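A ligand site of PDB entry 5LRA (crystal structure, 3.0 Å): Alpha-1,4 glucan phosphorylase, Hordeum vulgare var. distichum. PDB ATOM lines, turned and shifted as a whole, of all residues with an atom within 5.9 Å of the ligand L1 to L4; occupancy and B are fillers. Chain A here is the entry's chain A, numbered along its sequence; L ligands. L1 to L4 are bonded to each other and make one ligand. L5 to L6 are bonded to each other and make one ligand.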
ATOM      1  N   GLU A  93      32.395   2.166  -8.729  1.00  0.00           N
ATOM      2  CA  GLU A  93      32.718   0.867  -8.138  1.00  0.00           C
ATOM      3  C   GLU A  93      32.492  -0.258  -9.128  1.00  0.00           C
ATOM      4  O   GLU A  93      31.544  -0.205  -9.889  1.00  0.00           O
ATOM      5  CB  GLU A  93      31.802   0.592  -6.954  1.00  0.00           C
ATOM      6  CG  GLU A  93      32.064   1.374  -5.684  1.00  0.00           C
ATOM      7  CD  GLU A  93      31.206   0.864  -4.534  1.00  0.00           C
ATOM      8  OE1 GLU A  93      31.227  -0.346  -4.239  1.00  0.00           O
ATOM      9  OE2 GLU A  93      30.500   1.686  -3.921  1.00  0.00           O
ATOM     10  N   ASN A 138      33.713  -1.693  -3.319  1.00  0.00           N
ATOM     11  CA  ASN A 138      33.525  -1.581  -1.880  1.00  0.00           C
ATOM     12  C   ASN A 138      32.257  -2.307  -1.452  1.00  0.00           C
ATOM     13  O   ASN A 138      32.325  -3.318  -0.762  1.00  0.00           O
ATOM     14  CB  ASN A 138      33.471  -0.091  -1.506  1.00  0.00           C
ATOM     15  CG  ASN A 138      33.335   0.158  -0.008  1.00  0.00           C
ATOM     16  OD1 ASN A 138      33.087   1.283   0.419  1.00  0.00           O
ATOM     17  ND2 ASN A 138      33.525  -0.884   0.801  1.00  0.00           N
ATOM     18  N   GLY A 139      31.102  -1.819  -1.883  1.00  0.00           N
ATOM     19  CA  GLY A 139      29.824  -2.359  -1.416  1.00  0.00           C
ATOM     20  C   GLY A 139      28.926  -2.891  -2.514  1.00  0.00           C
ATOM     21  O   GLY A 139      29.402  -3.242  -3.607  1.00  0.00           O
ATOM     22  N   GLY A 140      27.626  -2.942  -2.206  1.00  0.00           N
ATOM     23  CA  GLY A 140      26.631  -3.426  -3.150  1.00  0.00           C
ATOM     24  C   GLY A 140      26.751  -2.737  -4.500  1.00  0.00           C
ATOM     25  O   GLY A 140      26.748  -3.390  -5.538  1.00  0.00           O
ATOM     26  N   LEU A 141      26.886  -1.416  -4.471  1.00  0.00           N
ATOM     27  CA  LEU A 141      26.953  -0.608  -5.685  1.00  0.00           C
ATOM     28  C   LEU A 141      27.883  -1.182  -6.717  1.00  0.00           C
ATOM     29  O   LEU A 141      27.620  -1.121  -7.917  1.00  0.00           O
ATOM     30  CB  LEU A 141      27.443   0.788  -5.354  1.00  0.00           C
ATOM     31  CG  LEU A 141      26.965   1.869  -6.310  1.00  0.00           C
ATOM     32  CD1 LEU A 141      25.751   2.550  -5.718  1.00  0.00           C
ATOM     33  CD2 LEU A 141      28.071   2.879  -6.583  1.00  0.00           C
ATOM     34  N   GLY A 142      29.015  -1.717  -6.236  1.00  0.00           N
ATOM     35  CA  GLY A 142      30.058  -2.256  -7.085  1.00  0.00           C
ATOM     36  C   GLY A 142      29.765  -3.664  -7.538  1.00  0.00           C
ATOM     37  O   GLY A 142      29.964  -4.000  -8.698  1.00  0.00           O
ATOM     38  N   LEU A 170      40.193   0.548  -1.964  1.00  0.00           N
ATOM     39  CA  LEU A 170      39.760   1.230  -0.766  1.00  0.00           C
ATOM     40  C   LEU A 170      40.772   0.962   0.351  1.00  0.00           C
ATOM     41  O   LEU A 170      41.406   1.900   0.844  1.00  0.00           O
ATOM     42  CB  LEU A 170      38.355   0.785  -0.367  1.00  0.00           C
ATOM     43  CG  LEU A 170      37.772   1.524   0.848  1.00  0.00           C
ATOM     44  CD1 LEU A 170      37.504   2.993   0.524  1.00  0.00           C
ATOM     45  CD2 LEU A 170      36.514   0.813   1.322  1.00  0.00           C
ATOM     46  N   TYR A 287      36.978   6.246  -3.247  1.00  0.00           N
ATOM     47  CA  TYR A 287      36.327   7.101  -2.254  1.00  0.00           C
ATOM     48  C   TYR A 287      37.333   7.688  -1.249  1.00  0.00           C
ATOM     49  O   TYR A 287      37.263   7.404  -0.042  1.00  0.00           O
ATOM     50  CB  TYR A 287      35.251   6.290  -1.500  1.00  0.00           C
ATOM     51  CG  TYR A 287      34.139   5.723  -2.362  1.00  0.00           C
ATOM     52  CD1 TYR A 287      33.669   6.410  -3.466  1.00  0.00           C
ATOM     53  CD2 TYR A 287      33.543   4.516  -2.040  1.00  0.00           C
ATOM     54  CE1 TYR A 287      32.663   5.898  -4.237  1.00  0.00           C
ATOM     55  CE2 TYR A 287      32.523   4.004  -2.808  1.00  0.00           C
ATOM     56  CZ  TYR A 287      32.082   4.699  -3.912  1.00  0.00           C
ATOM     57  OH  TYR A 287      31.074   4.226  -4.717  1.00  0.00           O
ATOM     58  N   ASP A 290      37.632  13.045   2.271  1.00  0.00           N
ATOM     59  CA  ASP A 290      37.295  14.348   1.713  1.00  0.00           C
ATOM     60  C   ASP A 290      36.879  15.393   2.743  1.00  0.00           C
ATOM     61  O   ASP A 290      36.176  16.347   2.413  1.00  0.00           O
ATOM     62  CB  ASP A 290      36.157  14.184   0.689  1.00  0.00           C
ATOM     63  CG  ASP A 290      34.845  13.725   1.340  1.00  0.00           C
ATOM     64  OD1 ASP A 290      34.857  13.356   2.542  1.00  0.00           O
ATOM     65  OD2 ASP A 290      33.803  13.720   0.638  1.00  0.00           O
ATOM     66  N   GLU A 291      37.310  15.230   3.996  1.00  0.00           N
ATOM     67  CA  GLU A 291      37.083  16.260   4.995  1.00  0.00           C
ATOM     68  C   GLU A 291      37.984  17.462   4.740  1.00  0.00           C
ATOM     69  O   GLU A 291      37.864  18.481   5.401  1.00  0.00           O
ATOM     70  CB  GLU A 291      37.335  15.716   6.403  1.00  0.00           C
ATOM     71  CG  GLU A 291      36.193  14.865   6.922  1.00  0.00           C
ATOM     72  CD  GLU A 291      36.595  14.006   8.117  1.00  0.00           C
ATOM     73  OE1 GLU A 291      35.899  13.000   8.375  1.00  0.00           O
ATOM     74  OE2 GLU A 291      37.592  14.338   8.795  1.00  0.00           O
ATOM     75  N   ARG A 299      38.174  14.010  -5.245  1.00  0.00           N
ATOM     76  CA  ARG A 299      36.931  13.260  -5.357  1.00  0.00           C
ATOM     77  C   ARG A 299      36.200  13.711  -6.619  1.00  0.00           C
ATOM     78  O   ARG A 299      35.628  12.907  -7.334  1.00  0.00           O
ATOM     79  CB  ARG A 299      36.064  13.527  -4.114  1.00  0.00           C
ATOM     80  CG  ARG A 299      34.965  12.529  -3.842  1.00  0.00           C
ATOM     81  CD  ARG A 299      35.518  11.250  -3.254  1.00  0.00           C
ATOM     82  NE  ARG A 299      35.414  11.166  -1.789  1.00  0.00           N
ATOM     83  CZ  ARG A 299      34.488  10.480  -1.093  1.00  0.00           C
ATOM     84  NH1 ARG A 299      33.527   9.811  -1.715  1.00  0.00           N
ATOM     85  NH2 ARG A 299      34.516  10.450   0.226  1.00  0.00           N
ATOM     86  N   ASP A 341      24.124   6.028  -9.132  1.00  0.00           N
ATOM     87  CA  ASP A 341      24.200   7.061  -8.076  1.00  0.00           C
ATOM     88  C   ASP A 341      24.677   8.403  -8.621  1.00  0.00           C
ATOM     89  O   ASP A 341      24.770   8.561  -9.832  1.00  0.00           O
ATOM     90  CB  ASP A 341      25.030   6.591  -6.890  1.00  0.00           C
ATOM     91  CG  ASP A 341      24.405   6.993  -5.555  1.00  0.00           C
ATOM     92  OD1 ASP A 341      24.242   8.207  -5.344  1.00  0.00           O
ATOM     93  OD2 ASP A 341      24.066   6.097  -4.756  1.00  0.00           O
ATOM     94  N   HIS A 343      27.563  10.051  -8.499  1.00  0.00           N
ATOM     95  CA  HIS A 343      28.966  10.277  -8.842  1.00  0.00           C
ATOM     96  C   HIS A 343      29.153  10.718 -10.311  1.00  0.00           C
ATOM     97  O   HIS A 343      29.887  11.680 -10.568  1.00  0.00           O
ATOM     98  CB  HIS A 343      29.823   9.048  -8.510  1.00  0.00           C
ATOM     99  CG  HIS A 343      29.623   8.519  -7.107  1.00  0.00           C
ATOM    100  ND1 HIS A 343      28.990   7.319  -6.853  1.00  0.00           N
ATOM    101  CD2 HIS A 343      29.978   9.028  -5.910  1.00  0.00           C
ATOM    102  CE1 HIS A 343      28.971   7.112  -5.542  1.00  0.00           C
ATOM    103  NE2 HIS A 343      29.566   8.135  -4.953  1.00  0.00           N
ATOM    104  N   HIS A 379      20.602   4.907  -5.227  1.00  0.00           N
ATOM    105  CA  HIS A 379      20.869   3.692  -4.454  1.00  0.00           C
ATOM    106  C   HIS A 379      20.759   3.799  -2.956  1.00  0.00           C
ATOM    107  O   HIS A 379      20.827   2.788  -2.266  1.00  0.00           O
ATOM    108  CB  HIS A 379      22.273   3.205  -4.754  1.00  0.00           C
ATOM    109  CG  HIS A 379      22.430   2.727  -6.153  1.00  0.00           C
ATOM    110  ND1 HIS A 379      22.252   1.403  -6.505  1.00  0.00           N
ATOM    111  CD2 HIS A 379      22.706   3.389  -7.296  1.00  0.00           C
ATOM    112  CE1 HIS A 379      22.436   1.273  -7.801  1.00  0.00           C
ATOM    113  NE2 HIS A 379      22.710   2.469  -8.300  1.00  0.00           N
ATOM    114  N   THR A 380      20.639   5.007  -2.429  1.00  0.00           N
ATOM    115  CA  THR A 380      20.432   5.168  -1.002  1.00  0.00           C
ATOM    116  C   THR A 380      19.967   6.568  -0.698  1.00  0.00           C
ATOM    117  O   THR A 380      20.554   7.560  -1.152  1.00  0.00           O
ATOM    118  CB  THR A 380      21.672   4.825  -0.111  1.00  0.00           C
ATOM    119  OG1 THR A 380      22.844   4.630  -0.922  1.00  0.00           O
ATOM    120  CG2 THR A 380      21.406   3.564   0.739  1.00  0.00           C
ATOM    121  N   LEU A 382      20.620   7.687   1.972  1.00  0.00           N
ATOM    122  CA  LEU A 382      21.773   8.196   2.787  1.00  0.00           C
ATOM    123  C   LEU A 382      22.537   9.383   2.142  1.00  0.00           C
ATOM    124  O   LEU A 382      22.899   9.312   0.967  1.00  0.00           O
ATOM    125  CB  LEU A 382      22.781   7.066   3.059  1.00  0.00           C
ATOM    126  CG  LEU A 382      22.722   6.211   4.335  1.00  0.00           C
ATOM    127  CD1 LEU A 382      22.875   7.073   5.585  1.00  0.00           C
ATOM    128  CD2 LEU A 382      21.452   5.370   4.415  1.00  0.00           C
ATOM    129  N   GLU A 384      25.546  10.762   2.130  1.00  0.00           N
ATOM    130  CA  GLU A 384      26.892  10.629   1.554  1.00  0.00           C
ATOM    131  C   GLU A 384      26.795  10.343   0.049  1.00  0.00           C
ATOM    132  O   GLU A 384      27.775  10.498  -0.705  1.00  0.00           O
ATOM    133  CB  GLU A 384      27.637   9.481   2.235  1.00  0.00           C
ATOM    134  CG  GLU A 384      27.494   9.422   3.757  1.00  0.00           C
ATOM    135  CD  GLU A 384      26.927   8.101   4.258  1.00  0.00           C
ATOM    136  OE1 GLU A 384      27.099   7.039   3.595  1.00  0.00           O
ATOM    137  OE2 GLU A 384      26.290   8.110   5.331  1.00  0.00           O
ATOM    138  N   ALA A 385      25.601   9.895  -0.388  1.00  0.00           N
ATOM    139  CA  ALA A 385      25.279   9.641  -1.794  1.00  0.00           C
ATOM    140  C   ALA A 385      24.541  10.829  -2.444  1.00  0.00           C
ATOM    141  O   ALA A 385      24.676  11.021  -3.658  1.00  0.00           O
ATOM    142  CB  ALA A 385      24.448   8.372  -1.913  1.00  0.00           C
ATOM    143  N   ARG A 657      29.262  -3.879   5.070  1.00  0.00           N
ATOM    144  CA  ARG A 657      29.905  -2.617   5.450  1.00  0.00           C
ATOM    145  C   ARG A 657      29.519  -2.230   6.879  1.00  0.00           C
ATOM    146  O   ARG A 657      28.347  -2.289   7.241  1.00  0.00           O
ATOM    147  CB  ARG A 657      29.554  -1.495   4.449  1.00  0.00           C
ATOM    148  CG  ARG A 657      29.785  -1.850   2.973  1.00  0.00           C
ATOM    149  CD  ARG A 657      29.752  -0.628   2.047  1.00  0.00           C
ATOM    150  NE  ARG A 657      28.436   0.033   1.985  1.00  0.00           N
ATOM    151  CZ  ARG A 657      28.067   1.101   2.710  1.00  0.00           C
ATOM    152  NH1 ARG A 657      26.842   1.608   2.550  1.00  0.00           N
ATOM    153  NH2 ARG A 657      28.895   1.683   3.571  1.00  0.00           N
ATOM    154  N   ILE A 658      30.493  -1.844   7.688  1.00  0.00           N
ATOM    155  CA  ILE A 658      30.277  -1.630   9.114  1.00  0.00           C
ATOM    156  C   ILE A 658      29.742  -0.221   9.368  1.00  0.00           C
ATOM    157  O   ILE A 658      30.488   0.752   9.329  1.00  0.00           O
ATOM    158  CB  ILE A 658      31.575  -1.833   9.927  1.00  0.00           C
ATOM    159  CG1 ILE A 658      32.189  -3.207   9.644  1.00  0.00           C
ATOM    160  CG2 ILE A 658      31.310  -1.652  11.421  1.00  0.00           C
ATOM    161  CD1 ILE A 658      31.297  -4.389  10.004  1.00  0.00           C
ATOM    162  N   HIS A 659      28.447  -0.126   9.617  1.00  0.00           N
ATOM    163  CA  HIS A 659      27.784   1.162   9.706  1.00  0.00           C
ATOM    164  C   HIS A 659      26.856   1.111  10.896  1.00  0.00           C
ATOM    165  O   HIS A 659      26.253   0.065  11.173  1.00  0.00           O
ATOM    166  CB  HIS A 659      26.994   1.417   8.413  1.00  0.00           C
ATOM    167  CG  HIS A 659      26.919   2.848   8.003  1.00  0.00           C
ATOM    168  ND1 HIS A 659      26.366   3.836   8.801  1.00  0.00           N
ATOM    169  CD2 HIS A 659      27.279   3.471   6.845  1.00  0.00           C
ATOM    170  CE1 HIS A 659      26.415   4.989   8.168  1.00  0.00           C
ATOM    171  NE2 HIS A 659      26.966   4.800   6.981  1.00  0.00           N
ATOM    172  N   GLU A 660      26.728   2.225  11.598  1.00  0.00           N
ATOM    173  CA  GLU A 660      25.810   2.301  12.720  1.00  0.00           C
ATOM    174  C   GLU A 660      24.422   1.803  12.284  1.00  0.00           C
ATOM    175  O   GLU A 660      23.759   1.110  13.057  1.00  0.00           O
ATOM    176  CB  GLU A 660      25.736   3.734  13.257  1.00  0.00           C
ATOM    177  CG  GLU A 660      26.998   4.195  13.998  1.00  0.00           C
ATOM    178  CD  GLU A 660      26.984   5.679  14.357  1.00  0.00           C
ATOM    179  OE1 GLU A 660      26.737   6.520  13.458  1.00  0.00           O
ATOM    180  OE2 GLU A 660      27.246   6.003  15.532  1.00  0.00           O
ATOM    181  N   TYR A 661      24.027   2.133  11.054  1.00  0.00           N
ATOM    182  CA  TYR A 661      22.664   1.851  10.562  1.00  0.00           C
ATOM    183  C   TYR A 661      22.418   0.406  10.150  1.00  0.00           C
ATOM    184  O   TYR A 661      21.274  -0.050  10.164  1.00  0.00           O
ATOM    185  CB  TYR A 661      22.297   2.816   9.404  1.00  0.00           C
ATOM    186  CG  TYR A 661      22.489   2.324   7.967  1.00  0.00           C
ATOM    187  CD1 TYR A 661      21.553   1.505   7.339  1.00  0.00           C
ATOM    188  CD2 TYR A 661      23.591   2.751   7.214  1.00  0.00           C
ATOM    189  CE1 TYR A 661      21.721   1.084   6.028  1.00  0.00           C
ATOM    190  CE2 TYR A 661      23.759   2.330   5.904  1.00  0.00           C
ATOM    191  CZ  TYR A 661      22.825   1.505   5.317  1.00  0.00           C
ATOM    192  OH  TYR A 661      22.998   1.092   4.029  1.00  0.00           O
ATOM    193  N   PHE A 702      34.596   2.241   7.214  1.00  0.00           N
ATOM    194  CA  PHE A 702      35.247   3.375   6.545  1.00  0.00           C
ATOM    195  C   PHE A 702      36.236   3.970   7.542  1.00  0.00           C
ATOM    196  O   PHE A 702      35.904   4.193   8.710  1.00  0.00           O
ATOM    197  CB  PHE A 702      34.235   4.421   6.015  1.00  0.00           C
ATOM    198  CG  PHE A 702      34.828   5.382   5.003  1.00  0.00           C
ATOM    199  CD1 PHE A 702      34.957   5.019   3.656  1.00  0.00           C
ATOM    200  CD2 PHE A 702      35.247   6.660   5.387  1.00  0.00           C
ATOM    201  CE1 PHE A 702      35.507   5.897   2.727  1.00  0.00           C
ATOM    202  CE2 PHE A 702      35.789   7.550   4.460  1.00  0.00           C
ATOM    203  CZ  PHE A 702      35.914   7.166   3.125  1.00  0.00           C
ATOM    204  N   THR A 704      37.840   6.595   8.377  1.00  0.00           N
ATOM    205  CA  THR A 704      37.706   7.865   9.075  1.00  0.00           C
ATOM    206  C   THR A 704      36.494   7.860  10.041  1.00  0.00           C
ATOM    207  O   THR A 704      36.456   8.604  11.033  1.00  0.00           O
ATOM    208  CB  THR A 704      37.660   9.012   8.018  1.00  0.00           C
ATOM    209  OG1 THR A 704      38.235  10.203   8.571  1.00  0.00           O
ATOM    210  CG2 THR A 704      36.245   9.278   7.495  1.00  0.00           C
ATOM    211  N   TYR A 705      35.529   6.972   9.760  1.00  0.00           N
ATOM    212  CA  TYR A 705      34.333   6.729  10.570  1.00  0.00           C
ATOM    213  C   TYR A 705      34.721   6.148  11.934  1.00  0.00           C
ATOM    214  O   TYR A 705      34.846   4.928  12.106  1.00  0.00           O
ATOM    215  CB  TYR A 705      33.408   5.756   9.810  1.00  0.00           C
ATOM    216  CG  TYR A 705      31.934   5.707  10.181  1.00  0.00           C
ATOM    217  CD1 TYR A 705      31.475   6.087  11.449  1.00  0.00           C
ATOM    218  CD2 TYR A 705      31.005   5.215   9.269  1.00  0.00           C
ATOM    219  CE1 TYR A 705      30.137   6.002  11.777  1.00  0.00           C
ATOM    220  CE2 TYR A 705      29.658   5.126   9.587  1.00  0.00           C
ATOM    221  CZ  TYR A 705      29.230   5.528  10.836  1.00  0.00           C
ATOM    222  OH  TYR A 705      27.885   5.455  11.166  1.00  0.00           O
ATOM    223  N   VAL A 706      34.899   7.039  12.908  1.00  0.00           N
ATOM    224  CA  VAL A 706      35.435   6.680  14.218  1.00  0.00           C
ATOM    225  C   VAL A 706      34.592   5.662  14.952  1.00  0.00           C
ATOM    226  O   VAL A 706      35.136   4.700  15.507  1.00  0.00           O
ATOM    227  CB  VAL A 706      35.559   7.917  15.128  1.00  0.00           C
ATOM    228  CG1 VAL A 706      35.996   7.498  16.535  1.00  0.00           C
ATOM    229  CG2 VAL A 706      36.515   8.931  14.510  1.00  0.00           C
ATOM    230  N   TYR A 858      23.729  14.960  18.470  1.00  0.00           N
ATOM    231  CA  TYR A 858      24.455  14.223  17.442  1.00  0.00           C
ATOM    232  C   TYR A 858      25.338  13.130  18.039  1.00  0.00           C
ATOM    233  O   TYR A 858      26.048  13.382  19.009  1.00  0.00           O
ATOM    234  CB  TYR A 858      25.336  15.180  16.613  1.00  0.00           C
ATOM    235  CG  TYR A 858      25.955  14.527  15.410  1.00  0.00           C
ATOM    236  CD1 TYR A 858      25.310  14.524  14.181  1.00  0.00           C
ATOM    237  CD2 TYR A 858      27.185  13.875  15.509  1.00  0.00           C
ATOM    238  CE1 TYR A 858      25.864  13.906  13.078  1.00  0.00           C
ATOM    239  CE2 TYR A 858      27.754  13.241  14.408  1.00  0.00           C
ATOM    240  CZ  TYR A 858      27.085  13.261  13.203  1.00  0.00           C
ATOM    241  OH  TYR A 858      27.642  12.642  12.116  1.00  0.00           O
ATOM    242  N   PHE A 864      19.604   5.080  15.635  1.00  0.00           N
ATOM    243  CA  PHE A 864      19.274   3.913  14.821  1.00  0.00           C
ATOM    244  C   PHE A 864      18.456   2.851  15.560  1.00  0.00           C
ATOM    245  O   PHE A 864      18.388   1.701  15.108  1.00  0.00           O
ATOM    246  CB  PHE A 864      20.541   3.333  14.251  1.00  0.00           C
ATOM    247  CG  PHE A 864      21.297   4.301  13.415  1.00  0.00           C
ATOM    248  CD1 PHE A 864      21.000   4.457  12.079  1.00  0.00           C
ATOM    249  CD2 PHE A 864      22.284   5.087  13.977  1.00  0.00           C
ATOM    250  CE1 PHE A 864      21.698   5.364  11.301  1.00  0.00           C
ATOM    251  CE2 PHE A 864      22.990   5.990  13.203  1.00  0.00           C
ATOM    252  CZ  PHE A 864      22.691   6.130  11.854  1.00  0.00           C
HETATM  253  C1  LIG L   1      30.730  10.391  10.400  1.00  0.00           C
HETATM  254  C2  LIG L   1      31.076  10.104   8.930  1.00  0.00           C
HETATM  255  C3  LIG L   1      30.234   8.965   8.357  1.00  0.00           C
HETATM  256  C4  LIG L   1      28.757   9.191   8.717  1.00  0.00           C
HETATM  257  C5  LIG L   1      27.840   8.116   8.139  1.00  0.00           C
HETATM  258  C6  LIG L   1      29.236  10.341  10.711  1.00  0.00           C
HETATM  259  O1  LIG L   1      29.023  10.302  12.119  1.00  0.00           O
HETATM  260  O2  LIG L   1      31.236  11.668  10.752  1.00  0.00           O
HETATM  261  O3  LIG L   1      32.446   9.815   8.858  1.00  0.00           O
HETATM  262  O4  LIG L   1      30.385   8.827   6.943  1.00  0.00           O
HETATM  263  O5  LIG L   1      28.630   9.203  10.126  1.00  0.00           O
HETATM  264  O6  LIG L   1      26.524   8.249   8.625  1.00  0.00           O
HETATM  265  C1  LG2 L   2      31.583   8.112   6.532  1.00  0.00           C
HETATM  266  C2  LG2 L   2      32.450   8.964   5.595  1.00  0.00           C
HETATM  267  C3  LG2 L   2      31.889   9.013   4.166  1.00  0.00           C
HETATM  268  C4  LG2 L   2      31.669   7.593   3.648  1.00  0.00           C
HETATM  269  C5  LG2 L   2      30.793   6.806   4.619  1.00  0.00           C
HETATM  270  C6  LG2 L   2      30.630   5.374   4.124  1.00  0.00           C
HETATM  271  O1  LG2 L   2      32.623  10.250   6.147  1.00  0.00           O
HETATM  272  O2  LG2 L   2      32.718   9.727   3.268  1.00  0.00           O
HETATM  273  O3  LG2 L   2      31.009   7.605   2.388  1.00  0.00           O
HETATM  274  O4  LG2 L   2      31.314   6.842   5.943  1.00  0.00           O
HETATM  275  O5  LG2 L   2      30.566   4.438   5.173  1.00  0.00           O
HETATM  276  C1  LG3 L   3      31.761   6.988   1.328  1.00  0.00           C
HETATM  277  C2  LG3 L   3      31.265   7.617   0.038  1.00  0.00           C
HETATM  278  C3  LG3 L   3      29.892   7.095  -0.301  1.00  0.00           C
HETATM  279  C4  LG3 L   3      30.032   5.601  -0.553  1.00  0.00           C
HETATM  280  C5  LG3 L   3      30.528   4.947   0.736  1.00  0.00           C
HETATM  281  C6  LG3 L   3      30.887   3.476   0.530  1.00  0.00           C
HETATM  282  O1  LG3 L   3      31.200   9.004   0.251  1.00  0.00           O
HETATM  283  O2  LG3 L   3      29.368   7.753  -1.424  1.00  0.00           O
HETATM  284  O3  LG3 L   3      28.747   5.099  -0.853  1.00  0.00           O
HETATM  285  O4  LG3 L   3      31.671   5.578   1.292  1.00  0.00           O
HETATM  286  O5  LG3 L   3      31.460   2.983   1.726  1.00  0.00           O
HETATM  287  C1  LG4 L   4      28.619   4.438  -2.124  1.00  0.00           C
HETATM  288  C2  LG4 L   4      27.240   4.777  -2.700  1.00  0.00           C
HETATM  289  C3  LG4 L   4      26.122   4.061  -1.962  1.00  0.00           C
HETATM  290  C4  LG4 L   4      26.385   2.556  -1.922  1.00  0.00           C
HETATM  291  C5  LG4 L   4      27.782   2.303  -1.347  1.00  0.00           C
HETATM  292  C6  LG4 L   4      28.147   0.808  -1.306  1.00  0.00           C
HETATM  293  O1  LG4 L   4      27.029   6.184  -2.619  1.00  0.00           O
HETATM  294  O2  LG4 L   4      24.877   4.358  -2.558  1.00  0.00           O
HETATM  295  O3  LG4 L   4      25.383   1.925  -1.136  1.00  0.00           O
HETATM  296  O4  LG4 L   4      28.787   3.028  -2.042  1.00  0.00           O
HETATM  297  O5  LG4 L   4      28.805   0.370  -2.467  1.00  0.00           O
HETATM  298  C1  LG5 L   5      20.571  16.289  13.644  1.00  0.00           C
HETATM  299  C2  LG5 L   5      20.572  15.502  14.969  1.00  0.00           C
HETATM  300  C3  LG5 L   5      21.304  14.158  14.826  1.00  0.00           C
HETATM  301  C4  LG5 L   5      21.070  13.420  13.493  1.00  0.00           C
HETATM  302  C5  LG5 L   5      20.559  14.319  12.365  1.00  0.00           C
HETATM  303  C6  LG5 L   5      19.677  13.532  11.400  1.00  0.00           C
HETATM  304  O1  LG5 L   5      21.907  16.756  13.647  1.00  0.00           O
HETATM  305  O2  LG5 L   5      21.127  16.279  16.024  1.00  0.00           O
HETATM  306  O3  LG5 L   5      20.876  13.297  15.877  1.00  0.00           O
HETATM  307  O4  LG5 L   5      22.277  12.834  13.043  1.00  0.00           O
HETATM  308  O5  LG5 L   5      19.788  15.401  12.879  1.00  0.00           O
HETATM  309  O6  LG5 L   5      19.062  14.462  10.552  1.00  0.00           O
HETATM  310  C1  LG6 L   6      22.186  11.391  12.999  1.00  0.00           C
HETATM  311  C2  LG6 L   6      22.602  10.762  14.354  1.00  0.00           C
HETATM  312  C3  LG6 L   6      24.037  10.217  14.442  1.00  0.00           C
HETATM  313  C4  LG6 L   6      24.439   9.544  13.139  1.00  0.00           C
HETATM  314  C5  LG6 L   6      24.219  10.491  11.959  1.00  0.00           C
HETATM  315  C6  LG6 L   6      24.663   9.873  10.626  1.00  0.00           C
HETATM  316  O1  LG6 L   6      22.401  11.641  15.448  1.00  0.00           O
HETATM  317  O2  LG6 L   6      24.165   9.328  15.543  1.00  0.00           O
HETATM  318  O3  LG6 L   6      25.795   9.128  13.219  1.00  0.00           O
HETATM  319  O4  LG6 L   6      22.854  10.854  11.867  1.00  0.00           O
HETATM  320  O5  LG6 L   6      25.619   8.842  10.778  1.00  0.00           O
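The guanidinium group (NH2) of Arg 657 lies within hydrogen-bond range of an oxygen (O5) of LG3 L3, at 3.4 Å. The backbone NH of Gly 139 sits close to an oxygen (O5) of LG4 L4, 3.2 Å away. An oxygen (O1) of LG3 L3 lies within hydrogen-bond range of the guanidinium group of Arg 299 (3.2 Å). OE2 of Glu 93 sits at hydrogen-bond distance from O5 of LG4 L4, at 2.6 Å. OE1 of Glu 660 lies within hydrogen-bond range of O3 of LG6 L6, 2.8 Å away. The side-chain carboxylate (OD2) of Asp 341 sits at hydrogen-bond distance from an oxygen (O2) of LG4 L4, 2.9 Å away. An oxygen (O5) of LG4 L4 lies close to the backbone NH (N) of Leu 141. O6 of LIG L1 lies close to OE2 of Glu 384 (3.3 Å). OG1 of Thr 380 sits at hydrogen-bond distance from O2 of LG4 L4 (2.6 Å). O5 of LG3 L3 lies within hydrogen-bond range of OD1 of Asn 138 (2.7 Å). The backbone carbonyl oxygen (O) of Glu 384 lies within hydrogen-bond range of an oxygen (O2) of LG3 L3, at 3.3 Å. The side-chain hydroxyl (OH) of Tyr 858 lies within hydrogen-bond range of an oxygen (O1) of LIG L1 (2.7 Å).
O6 of LIG L1 lies within hydrogen-bond range of O5 of LG6 L6, 2.4 Å away.
OE1 of Glu 660 lies within hydrogen-bond range of OH of Tyr 705 (2.8 Å). The side-chain carboxylate (OE1) of Glu 93 sits at hydrogen-bond distance from the backbone NH (N) of Asn 138, at 3.0 Å. The side-chain hydroxyl (OH) of Tyr 705 lies within hydrogen-bond range of a ring nitrogen (ND1) of His 659, at 3.2 Å. The side-chain carboxylate (OE1) of Glu 93 lies within hydrogen-bond range of the backbone NH (N) of Gly 142. OH of Tyr 287 sits at hydrogen-bond distance from OE2 of Glu 93 (2.7 Å). The side-chain carboxylate of Glu 93 lies within hydrogen-bond range of the backbone NH of Gly 139 (2.8 Å). The guanidinium group of Arg 299 is in salt-bridge range of the side-chain carboxylate of Asp 290, at 3.4 Å.
N of Gly 140 touches O5 of LG4 L4, 3.5 Å away. OH of Tyr 287 touches C1 of LG4 L4, at 3.6 Å. NE2 of His 343 touches O2 of LG3 L3, 3.6 Å away. His 379 touches the ligand L1 to L4. Ala 385 touches the ligand L1 to L4. CE1 of His 659 touches O6 of LIG L1, at 3.3 Å. CD2 of Phe 702 touches C2 of LG2 L2, at 3.6 Å. Thr 704 touches the ligand L1 to L4. CD2 of Tyr 705 touches O4 of LG2 L2 (3.7 Å). Hydrophobic or aromatic side chains within 4 Å of the ligand L1 to L4: Leu 141, Tyr 287, His 343, His 379, Ala 385, His 659, Phe 702, Tyr 705 and Tyr 858. Within 4 Å of the ligand L1 to L4: Glu 93, Asn 138, Gly 139, Gly 140, Leu 141, Tyr 287, Arg 299, Asp 341, His 343, His 379, Thr 380, Glu 384, Ala 385, Arg 657, His 659, Phe 702, Thr 704, Tyr 705 and Tyr 858. The nearest printed residue that does not touch the ligand L1 to L4 is Asp 290 (4.3 Å).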
